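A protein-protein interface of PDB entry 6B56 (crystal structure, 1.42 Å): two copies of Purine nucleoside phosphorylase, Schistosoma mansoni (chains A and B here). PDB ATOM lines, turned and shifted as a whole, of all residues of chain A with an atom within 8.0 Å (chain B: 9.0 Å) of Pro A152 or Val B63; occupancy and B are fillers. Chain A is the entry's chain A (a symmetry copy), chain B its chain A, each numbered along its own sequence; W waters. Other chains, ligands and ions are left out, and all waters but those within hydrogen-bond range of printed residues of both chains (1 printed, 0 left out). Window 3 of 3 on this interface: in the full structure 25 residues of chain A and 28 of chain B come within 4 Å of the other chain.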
ATOM      1  N   VAL A   6      13.597  36.371  -7.388  1.00  0.00           N
ATOM      2  CA  VAL A   6      12.981  35.054  -7.276  1.00  0.00           C
ATOM      3  C   VAL A   6      11.515  35.189  -6.863  1.00  0.00           C
ATOM      4  O   VAL A   6      11.144  36.080  -6.074  1.00  0.00           O
ATOM      5  CB  VAL A   6      13.783  34.190  -6.276  1.00  0.00           C
ATOM      6  CG1 VAL A   6      13.142  32.823  -5.985  1.00  0.00           C
ATOM      7  CG2 VAL A   6      15.197  33.991  -6.816  1.00  0.00           C
ATOM      8  N   ALA A   7      10.664  34.294  -7.387  1.00  0.00           N
ATOM      9  CA  ALA A   7       9.239  34.259  -7.043  1.00  0.00           C
ATOM     10  C   ALA A   7       9.017  33.508  -5.723  1.00  0.00           C
ATOM     11  O   ALA A   7       8.277  32.520  -5.632  1.00  0.00           O
ATOM     12  CB  ALA A   7       8.448  33.624  -8.178  1.00  0.00           C
ATOM     13  N   GLN A  96      10.938  32.713 -13.067  1.00  0.00           N
ATOM     14  CA  GLN A  96      10.604  33.485 -11.868  1.00  0.00           C
ATOM     15  C   GLN A  96       9.734  34.693 -12.217  1.00  0.00           C
ATOM     16  O   GLN A  96       8.860  35.080 -11.425  1.00  0.00           O
ATOM     17  CB  GLN A  96      11.868  33.963 -11.152  1.00  0.00           C
ATOM     18  CG  GLN A  96      12.912  32.868 -10.862  1.00  0.00           C
ATOM     19  CD  GLN A  96      12.473  31.940  -9.737  1.00  0.00           C
ATOM     20  OE1 GLN A  96      11.442  32.138  -9.106  1.00  0.00           O
ATOM     21  NE2 GLN A  96      13.271  30.898  -9.493  1.00  0.00           N
ATOM     22  N   ARG A 103       1.564  34.074  -8.146  1.00  0.00           N
ATOM     23  CA  ARG A 103       1.726  33.871  -6.703  1.00  0.00           C
ATOM     24  C   ARG A 103       1.242  35.076  -5.891  1.00  0.00           C
ATOM     25  O   ARG A 103       0.718  34.901  -4.783  1.00  0.00           O
ATOM     26  CB  ARG A 103       3.187  33.472  -6.432  1.00  0.00           C
ATOM     27  CG  ARG A 103       3.471  32.022  -6.885  1.00  0.00           C
ATOM     28  CD  ARG A 103       4.936  31.572  -6.706  1.00  0.00           C
ATOM     29  NE  ARG A 103       5.066  30.156  -7.055  1.00  0.00           N
ATOM     30  CZ  ARG A 103       6.209  29.507  -7.235  1.00  0.00           C
ATOM     31  NH1 ARG A 103       7.376  30.125  -7.114  1.00  0.00           N
ATOM     32  NH2 ARG A 103       6.185  28.240  -7.606  1.00  0.00           N
ATOM     33  N   VAL A 148       8.230  25.545 -16.201  1.00  0.00           N
ATOM     34  CA  VAL A 148       8.169  26.782 -15.388  1.00  0.00           C
ATOM     35  C   VAL A 148       8.590  26.570 -13.931  1.00  0.00           C
ATOM     36  O   VAL A 148       8.953  27.539 -13.237  1.00  0.00           O
ATOM     37  CB  VAL A 148       6.742  27.405 -15.514  1.00  0.00           C
ATOM     38  CG1 VAL A 148       5.689  26.549 -14.786  1.00  0.00           C
ATOM     39  CG2 VAL A 148       6.713  28.880 -15.046  1.00  0.00           C
ATOM     40  N   LEU A 149       8.549  25.329 -13.437  1.00  0.00           N
ATOM     41  CA  LEU A 149       8.932  25.001 -12.059  1.00  0.00           C
ATOM     42  C   LEU A 149      10.394  24.548 -11.895  1.00  0.00           C
ATOM     43  O   LEU A 149      10.806  24.210 -10.772  1.00  0.00           O
ATOM     44  CB  LEU A 149       7.948  23.973 -11.460  1.00  0.00           C
ATOM     45  CG  LEU A 149       6.551  24.524 -11.052  1.00  0.00           C
ATOM     46  CD1 LEU A 149       5.640  23.380 -10.645  1.00  0.00           C
ATOM     47  CD2 LEU A 149       6.641  25.540  -9.910  1.00  0.00           C
ATOM     48  N   VAL A 150      11.201  24.491 -12.969  1.00  0.00           N
ATOM     49  CA  VAL A 150      12.625  24.159 -12.810  1.00  0.00           C
ATOM     50  C   VAL A 150      13.308  25.216 -11.952  1.00  0.00           C
ATOM     51  O   VAL A 150      13.221  26.419 -12.228  1.00  0.00           O
ATOM     52  CB  VAL A 150      13.325  24.015 -14.178  1.00  0.00           C
ATOM     53  CG1 VAL A 150      14.842  23.877 -14.024  1.00  0.00           C
ATOM     54  CG2 VAL A 150      12.781  22.803 -14.951  1.00  0.00           C
ATOM     55  N   GLY A 151      14.026  24.756 -10.917  1.00  0.00           N
ATOM     56  CA  GLY A 151      14.617  25.610  -9.910  1.00  0.00           C
ATOM     57  C   GLY A 151      14.285  25.097  -8.520  1.00  0.00           C
ATOM     58  O   GLY A 151      13.608  24.071  -8.357  1.00  0.00           O
ATOM     59  N   PRO A 152      14.781  25.779  -7.489  1.00  0.00           N
ATOM     60  CA  PRO A 152      14.373  25.439  -6.122  1.00  0.00           C
ATOM     61  C   PRO A 152      12.860  25.492  -5.996  1.00  0.00           C
ATOM     62  O   PRO A 152      12.210  26.361  -6.577  1.00  0.00           O
ATOM     63  CB  PRO A 152      15.033  26.537  -5.273  1.00  0.00           C
ATOM     64  CG  PRO A 152      16.076  27.190  -6.151  1.00  0.00           C
ATOM     65  CD  PRO A 152      15.634  26.985  -7.558  1.00  0.00           C
ATOM     66  N   ASN A 153      12.292  24.590  -5.186  1.00  0.00           N
ATOM     67  CA  ASN A 153      10.860  24.702  -4.890  1.00  0.00           C
ATOM     68  C   ASN A 153      10.633  25.779  -3.838  1.00  0.00           C
ATOM     69  O   ASN A 153      11.384  25.880  -2.856  1.00  0.00           O
ATOM     70  CB  ASN A 153      10.271  23.374  -4.386  1.00  0.00           C
ATOM     71  CG  ASN A 153       8.737  23.405  -4.312  1.00  0.00           C
ATOM     72  OD1 ASN A 153       8.043  23.649  -5.323  1.00  0.00           O
ATOM     73  ND2 ASN A 153       8.203  23.167  -3.116  1.00  0.00           N
ATOM     74  N   GLN A 154       9.551  26.547  -4.016  1.00  0.00           N
ATOM     75  CA  GLN A 154       9.088  27.526  -3.019  1.00  0.00           C
ATOM     76  C   GLN A 154       7.979  26.847  -2.202  1.00  0.00           C
ATOM     77  O   GLN A 154       6.796  26.851  -2.579  1.00  0.00           O
ATOM     78  CB  GLN A 154       8.648  28.831  -3.686  1.00  0.00           C
ATOM     79  CG  GLN A 154       9.765  29.468  -4.575  1.00  0.00           C
ATOM     80  CD  GLN A 154      11.079  29.742  -3.840  1.00  0.00           C
ATOM     81  OE1 GLN A 154      11.117  30.006  -2.627  1.00  0.00           O
ATOM     82  NE2 GLN A 154      12.182  29.694  -4.586  1.00  0.00           N
ATOM     83  N   ASP A 155       8.395  26.237  -1.070  1.00  0.00           N
ATOM     84  CA  ASP A 155       7.548  25.330  -0.285  1.00  0.00           C
ATOM     85  C   ASP A 155       6.255  25.993   0.221  1.00  0.00           C
ATOM     86  O   ASP A 155       5.217  25.314   0.373  1.00  0.00           O
ATOM     87  CB  ASP A 155       8.341  24.764   0.912  1.00  0.00           C
ATOM     88  CG  ASP A 155       9.528  23.878   0.502  1.00  0.00           C
ATOM     89  OD1 ASP A 155       9.512  23.219  -0.543  1.00  0.00           O
ATOM     90  OD2 ASP A 155      10.489  23.763   1.291  1.00  0.00           O
ATOM     91  N   ARG A 160       7.045  19.906  -4.091  1.00  0.00           N
ATOM     92  CA  ARG A 160       8.158  19.745  -5.042  1.00  0.00           C
ATOM     93  C   ARG A 160       7.713  19.096  -6.351  1.00  0.00           C
ATOM     94  O   ARG A 160       8.178  19.499  -7.437  1.00  0.00           O
ATOM     95  CB  ARG A 160       9.295  18.947  -4.383  1.00  0.00           C
ATOM     96  CG  ARG A 160      10.431  18.473  -5.317  1.00  0.00           C
ATOM     97  CD  ARG A 160      11.437  19.570  -5.704  1.00  0.00           C
ATOM     98  NE  ARG A 160      10.936  20.496  -6.718  1.00  0.00           N
ATOM     99  CZ  ARG A 160      11.672  21.453  -7.296  1.00  0.00           C
ATOM    100  NH1 ARG A 160      12.970  21.575  -6.974  1.00  0.00           N
ATOM    101  NH2 ARG A 160      11.129  22.264  -8.204  1.00  0.00           N
ATOM    102  N   HIS A 232      -0.013  24.398  -8.888  1.00  0.00           N
ATOM    103  CA  HIS A 232       0.944  24.191  -7.797  1.00  0.00           C
ATOM    104  C   HIS A 232       0.459  24.812  -6.487  1.00  0.00           C
ATOM    105  O   HIS A 232       0.594  24.182  -5.430  1.00  0.00           O
ATOM    106  CB  HIS A 232       2.316  24.736  -8.249  1.00  0.00           C
ATOM    107  CG  HIS A 232       3.425  24.660  -7.227  1.00  0.00           C
ATOM    108  ND1 HIS A 232       3.846  25.775  -6.519  1.00  0.00           N
ATOM    109  CD2 HIS A 232       4.278  23.662  -6.888  1.00  0.00           C
ATOM    110  CE1 HIS A 232       4.869  25.449  -5.751  1.00  0.00           C
ATOM    111  NE2 HIS A 232       5.162  24.173  -5.963  1.00  0.00           N
ATOM    112  N   PRO B  59      29.788  20.648  -6.283  1.00  0.00           N
ATOM    113  CA  PRO B  59      28.703  21.639  -6.248  1.00  0.00           C
ATOM    114  C   PRO B  59      28.132  21.809  -4.851  1.00  0.00           C
ATOM    115  O   PRO B  59      28.125  20.879  -4.043  1.00  0.00           O
ATOM    116  CB  PRO B  59      27.649  21.055  -7.190  1.00  0.00           C
ATOM    117  CG  PRO B  59      27.963  19.583  -7.279  1.00  0.00           C
ATOM    118  CD  PRO B  59      29.441  19.434  -7.031  1.00  0.00           C
ATOM    119  N   LYS B  60      27.652  23.022  -4.595  1.00  0.00           N
ATOM    120  CA  LYS B  60      26.922  23.334  -3.375  1.00  0.00           C
ATOM    121  C   LYS B  60      25.562  22.642  -3.425  1.00  0.00           C
ATOM    122  O   LYS B  60      24.891  22.659  -4.462  1.00  0.00           O
ATOM    123  CB  LYS B  60      26.728  24.851  -3.309  1.00  0.00           C
ATOM    124  CG  LYS B  60      26.199  25.382  -2.013  1.00  0.00           C
ATOM    125  CD  LYS B  60      27.336  25.902  -1.125  1.00  0.00           C
ATOM    126  CE  LYS B  60      26.814  26.328   0.242  1.00  0.00           C
ATOM    127  NZ  LYS B  60      27.633  25.754   1.352  1.00  0.00           N
ATOM    128  N   THR B  61      25.150  22.026  -2.304  1.00  0.00           N
ATOM    129  CA  THR B  61      23.926  21.222  -2.260  1.00  0.00           C
ATOM    130  C   THR B  61      23.066  21.551  -1.041  1.00  0.00           C
ATOM    131  O   THR B  61      22.459  20.651  -0.456  1.00  0.00           O
ATOM    132  CB  THR B  61      24.226  19.723  -2.303  1.00  0.00           C
ATOM    133  OG1 THR B  61      25.032  19.325  -1.176  1.00  0.00           O
ATOM    134  CG2 THR B  61      24.955  19.373  -3.589  1.00  0.00           C
ATOM    135  N   THR B  62      22.974  22.836  -0.667  1.00  0.00           N
ATOM    136  CA  THR B  62      22.166  23.266   0.485  1.00  0.00           C
ATOM    137  C   THR B  62      20.993  24.184   0.165  1.00  0.00           C
ATOM    138  O   THR B  62      20.308  24.619   1.103  1.00  0.00           O
ATOM    139  CB  THR B  62      22.998  24.050   1.497  1.00  0.00           C
ATOM    140  OG1 THR B  62      23.378  25.296   0.901  1.00  0.00           O
ATOM    141  CG2 THR B  62      24.203  23.265   1.955  1.00  0.00           C
ATOM    142  N   VAL B  63      20.776  24.578  -1.087  1.00  0.00           N
ATOM    143  CA  VAL B  63      19.527  25.267  -1.409  1.00  0.00           C
ATOM    144  C   VAL B  63      18.370  24.276  -1.339  1.00  0.00           C
ATOM    145  O   VAL B  63      17.387  24.469  -0.603  1.00  0.00           O
ATOM    146  CB  VAL B  63      19.620  25.964  -2.781  1.00  0.00           C
ATOM    147  CG1 VAL B  63      18.238  26.342  -3.281  1.00  0.00           C
ATOM    148  CG2 VAL B  63      20.492  27.226  -2.693  1.00  0.00           C
ATOM    149  N   ALA B  64      18.488  23.187  -2.098  1.00  0.00           N
ATOM    150  CA  ALA B  64      17.586  22.055  -1.945  1.00  0.00           C
ATOM    151  C   ALA B  64      17.706  21.443  -0.560  1.00  0.00           C
ATOM    152  O   ALA B  64      16.740  20.861  -0.048  1.00  0.00           O
ATOM    153  CB  ALA B  64      17.924  20.999  -2.996  1.00  0.00           C
ATOM    154  N   GLY B  65      18.880  21.549   0.054  1.00  0.00           N
ATOM    155  CA  GLY B  65      19.076  21.032   1.390  1.00  0.00           C
ATOM    156  C   GLY B  65      19.230  19.521   1.405  1.00  0.00           C
ATOM    157  O   GLY B  65      19.566  18.875   0.400  1.00  0.00           O
ATOM    158  N   HIS B  66      18.983  18.946   2.583  1.00  0.00           N
ATOM    159  CA  HIS B  66      19.104  17.499   2.740  1.00  0.00           C
ATOM    160  C   HIS B  66      20.530  17.002   2.487  1.00  0.00           C
ATOM    161  O   HIS B  66      21.464  17.805   2.363  1.00  0.00           O
ATOM    162  CB  HIS B  66      18.044  16.830   1.864  1.00  0.00           C
ATOM    163  CG  HIS B  66      16.662  17.368   2.104  1.00  0.00           C
ATOM    164  ND1 HIS B  66      15.840  16.881   3.098  1.00  0.00           N
ATOM    165  CD2 HIS B  66      15.974  18.373   1.508  1.00  0.00           C
ATOM    166  CE1 HIS B  66      14.699  17.550   3.095  1.00  0.00           C
ATOM    167  NE2 HIS B  66      14.755  18.462   2.141  1.00  0.00           N
ATOM    168  N   ARG B  86      20.938  13.954  -3.527  1.00  0.00           N
ATOM    169  CA  ARG B  86      20.171  14.063  -4.761  1.00  0.00           C
ATOM    170  C   ARG B  86      20.708  15.243  -5.553  1.00  0.00           C
ATOM    171  O   ARG B  86      20.814  16.346  -5.007  1.00  0.00           O
ATOM    172  CB  ARG B  86      18.691  14.267  -4.425  1.00  0.00           C
ATOM    173  CG  ARG B  86      17.772  14.232  -5.636  1.00  0.00           C
ATOM    174  CD  ARG B  86      16.318  14.419  -5.217  1.00  0.00           C
ATOM    175  NE  ARG B  86      15.974  15.833  -5.070  1.00  0.00           N
ATOM    176  CZ  ARG B  86      14.863  16.280  -4.486  1.00  0.00           C
ATOM    177  NH1 ARG B  86      13.983  15.428  -3.964  1.00  0.00           N
ATOM    178  NH2 ARG B  86      14.639  17.587  -4.402  1.00  0.00           N
ATOM    179  N   HIS B  88      19.496  16.465  -9.137  1.00  0.00           N
ATOM    180  CA  HIS B  88      18.602  16.327 -10.283  1.00  0.00           C
ATOM    181  C   HIS B  88      18.440  17.647 -11.041  1.00  0.00           C
ATOM    182  O   HIS B  88      18.495  18.745 -10.469  1.00  0.00           O
ATOM    183  CB  HIS B  88      17.249  15.760  -9.855  1.00  0.00           C
ATOM    184  CG  HIS B  88      17.316  14.330  -9.399  1.00  0.00           C
ATOM    185  ND1 HIS B  88      16.240  13.689  -8.839  1.00  0.00           N
ATOM    186  CD2 HIS B  88      18.327  13.425  -9.411  1.00  0.00           C
ATOM    187  CE1 HIS B  88      16.574  12.452  -8.518  1.00  0.00           C
ATOM    188  NE2 HIS B  88      17.835  12.263  -8.860  1.00  0.00           N
ATOM    189  N   MET B  89      18.226  17.542 -12.359  1.00  0.00           N
ATOM    190  CA  MET B  89      18.252  18.746 -13.181  1.00  0.00           C
ATOM    191  C   MET B  89      17.011  19.618 -12.980  1.00  0.00           C
ATOM    192  O   MET B  89      17.096  20.845 -13.167  1.00  0.00           O
ATOM    193  CB  MET B  89      18.499  18.391 -14.651  1.00  0.00           C
ATOM    194  CG  MET B  89      19.794  17.581 -14.831  1.00  0.00           C
ATOM    195  SD  MET B  89      20.662  17.666 -16.413  1.00  0.00           S
ATOM    196  CE  MET B  89      21.087  19.409 -16.385  1.00  0.00           C
ATOM    197  N   TYR B  90      15.873  19.041 -12.560  1.00  0.00           N
ATOM    198  CA  TYR B  90      14.695  19.869 -12.267  1.00  0.00           C
ATOM    199  C   TYR B  90      14.946  20.834 -11.100  1.00  0.00           C
ATOM    200  O   TYR B  90      14.153  21.765 -10.898  1.00  0.00           O
ATOM    201  CB  TYR B  90      13.433  19.024 -12.004  1.00  0.00           C
ATOM    202  CG  TYR B  90      13.578  18.006 -10.895  1.00  0.00           C
ATOM    203  CD1 TYR B  90      13.567  18.392  -9.545  1.00  0.00           C
ATOM    204  CD2 TYR B  90      13.747  16.660 -11.186  1.00  0.00           C
ATOM    205  CE1 TYR B  90      13.741  17.450  -8.534  1.00  0.00           C
ATOM    206  CE2 TYR B  90      13.940  15.720 -10.177  1.00  0.00           C
ATOM    207  CZ  TYR B  90      13.926  16.125  -8.864  1.00  0.00           C
ATOM    208  OH  TYR B  90      14.123  15.189  -7.873  1.00  0.00           O
ATOM    209  N   GLU B  91      16.006  20.618 -10.298  1.00  0.00           N
ATOM    210  CA  GLU B  91      16.334  21.523  -9.192  1.00  0.00           C
ATOM    211  C   GLU B  91      17.080  22.773  -9.647  1.00  0.00           C
ATOM    212  O   GLU B  91      17.251  23.690  -8.819  1.00  0.00           O
ATOM    213  CB  GLU B  91      17.189  20.810  -8.125  1.00  0.00           C
ATOM    214  CG  GLU B  91      16.475  19.746  -7.333  1.00  0.00           C
ATOM    215  CD  GLU B  91      15.604  20.304  -6.143  1.00  0.00           C
ATOM    216  OE1 GLU B  91      15.795  21.452  -5.655  1.00  0.00           O
ATOM    217  OE2 GLU B  91      14.709  19.573  -5.673  1.00  0.00           O
ATOM    218  N   GLY B  92      17.525  22.826 -10.910  1.00  0.00           N
ATOM    219  CA  GLY B  92      18.254  23.971 -11.451  1.00  0.00           C
ATOM    220  C   GLY B  92      19.771  23.820 -11.516  1.00  0.00           C
ATOM    221  O   GLY B  92      20.449  24.789 -11.896  1.00  0.00           O
ATOM    222  N   TYR B  93      20.319  22.661 -11.152  1.00  0.00           N
ATOM    223  CA  TYR B  93      21.756  22.403 -11.292  1.00  0.00           C
ATOM    224  C   TYR B  93      22.137  22.436 -12.772  1.00  0.00           C
ATOM    225  O   TYR B  93      21.352  22.054 -13.649  1.00  0.00           O
ATOM    226  CB  TYR B  93      22.119  21.022 -10.697  1.00  0.00           C
ATOM    227  CG  TYR B  93      21.973  20.897  -9.176  1.00  0.00           C
ATOM    228  CD1 TYR B  93      22.866  21.531  -8.318  1.00  0.00           C
ATOM    229  CD2 TYR B  93      20.953  20.128  -8.593  1.00  0.00           C
ATOM    230  CE1 TYR B  93      22.730  21.430  -6.923  1.00  0.00           C
ATOM    231  CE2 TYR B  93      20.813  20.033  -7.219  1.00  0.00           C
ATOM    232  CZ  TYR B  93      21.696  20.677  -6.382  1.00  0.00           C
ATOM    233  OH  TYR B  93      21.544  20.548  -5.009  1.00  0.00           O
ATOM    234  N   PRO B 200       9.689  19.358 -12.814  1.00  0.00           N
ATOM    235  CA  PRO B 200       9.334  18.440 -11.706  1.00  0.00           C
ATOM    236  C   PRO B 200       7.857  18.045 -11.628  1.00  0.00           C
ATOM    237  O   PRO B 200       7.488  17.315 -10.690  1.00  0.00           O
ATOM    238  CB  PRO B 200       9.712  19.258 -10.459  1.00  0.00           C
ATOM    239  CG  PRO B 200       9.388  20.682 -10.868  1.00  0.00           C
ATOM    240  CD  PRO B 200       9.745  20.756 -12.354  1.00  0.00           C
HETATM  241  O   HOH W   1      13.880  22.702  -3.557  1.00  0.00           O
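Of chain B, only Val B63 and Glu B91 come within 4 Å of Pro A152.
No residue of chain A comes within 4 Å of Ala B64.
Printed residues of chain A within 4 Å of Met B89: Val A150.
Printed residues of chain B within 4 Å of Leu A149: Pro B200 (3.6 Å).
Of the printed residues of chain B, Gly A151 touches Tyr B90 (3.0 Å), Glu B91 (3.3 Å) and Gly B92 (3.996 Å).
Thr B62 touches none of the printed residues of chain A.
The nearest printed residue of chain B that does not touch Pro A152 is Gly B92 (5.3 Å).
Leu A149 touches Pro B200 (CB to CG, 3.6 Å).
Val A150 touches Met B89.
Val A150 touches Tyr B90.
Glu B91 touches Gly A151.
N of Gly B92 touches N of Gly A151, 3.996 Å away.
CG of Pro A152 touches CG1 of Val B63 (3.7 Å).
Arg A160 touches Arg B86.
Pro B200 touches Arg A160.
Printed residues of chain B that touch a printed residue of chain A: Val B63, Arg B86, Met B89, Tyr B90, Glu B91, Gly B92 and Pro B200.
Hydrophobic or aromatic side chains of chain B within 4 Å of the printed part of chain A: Val B63 and Pro B200.
Of the 14 printed residues of chain A, 5 touch a printed residue of chain B.
Hydrophobic or aromatic side chains of chain A within 4 Å of the printed part of chain B: Leu A149, Val A150 and Pro A152.
Along chain A the printed residues that touch a printed residue of chain B span positions 149 to 160.
Among the printed residues, 11 pairs touch across the chains.
Water W1 bridges the backbone NH of Asn A153 (3.0 Å) and the side-chain carboxylate of Glu B91 (3.1 Å).
The backbone carbonyl oxygen (O) of Tyr B90 sits at hydrogen-bond distance from the backbone NH (N) of Gly A151 (3.0 Å).
The guanidinium group (NH1) of Arg A160 lies within salt-bridge range of the side-chain carboxylate (OE2) of Glu B91 (3.0 Å).
O of Glu B91 lies close to N of Pro A152, 3.5 Å away.
NE of Arg B86 sits at hydrogen-bond distance from OH of Tyr B90 (3.4 Å).
NE of Arg B86 lies within salt-bridge range of OE2 of Glu B91.
ND1 of His B88 sits at hydrogen-bond distance from OH of Tyr B90.
O of Leu A149 is in hydrogen-bond range of NH2 of Arg A160, at 3.2 Å.
O of Gly A151 sits at hydrogen-bond distance from NH1 of Arg A160 (2.9 Å).
No position is printed for both chains.
Of the 11 pairs that touch across the chains among the printed residues, none has its exchanged pair printed and touching as well.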
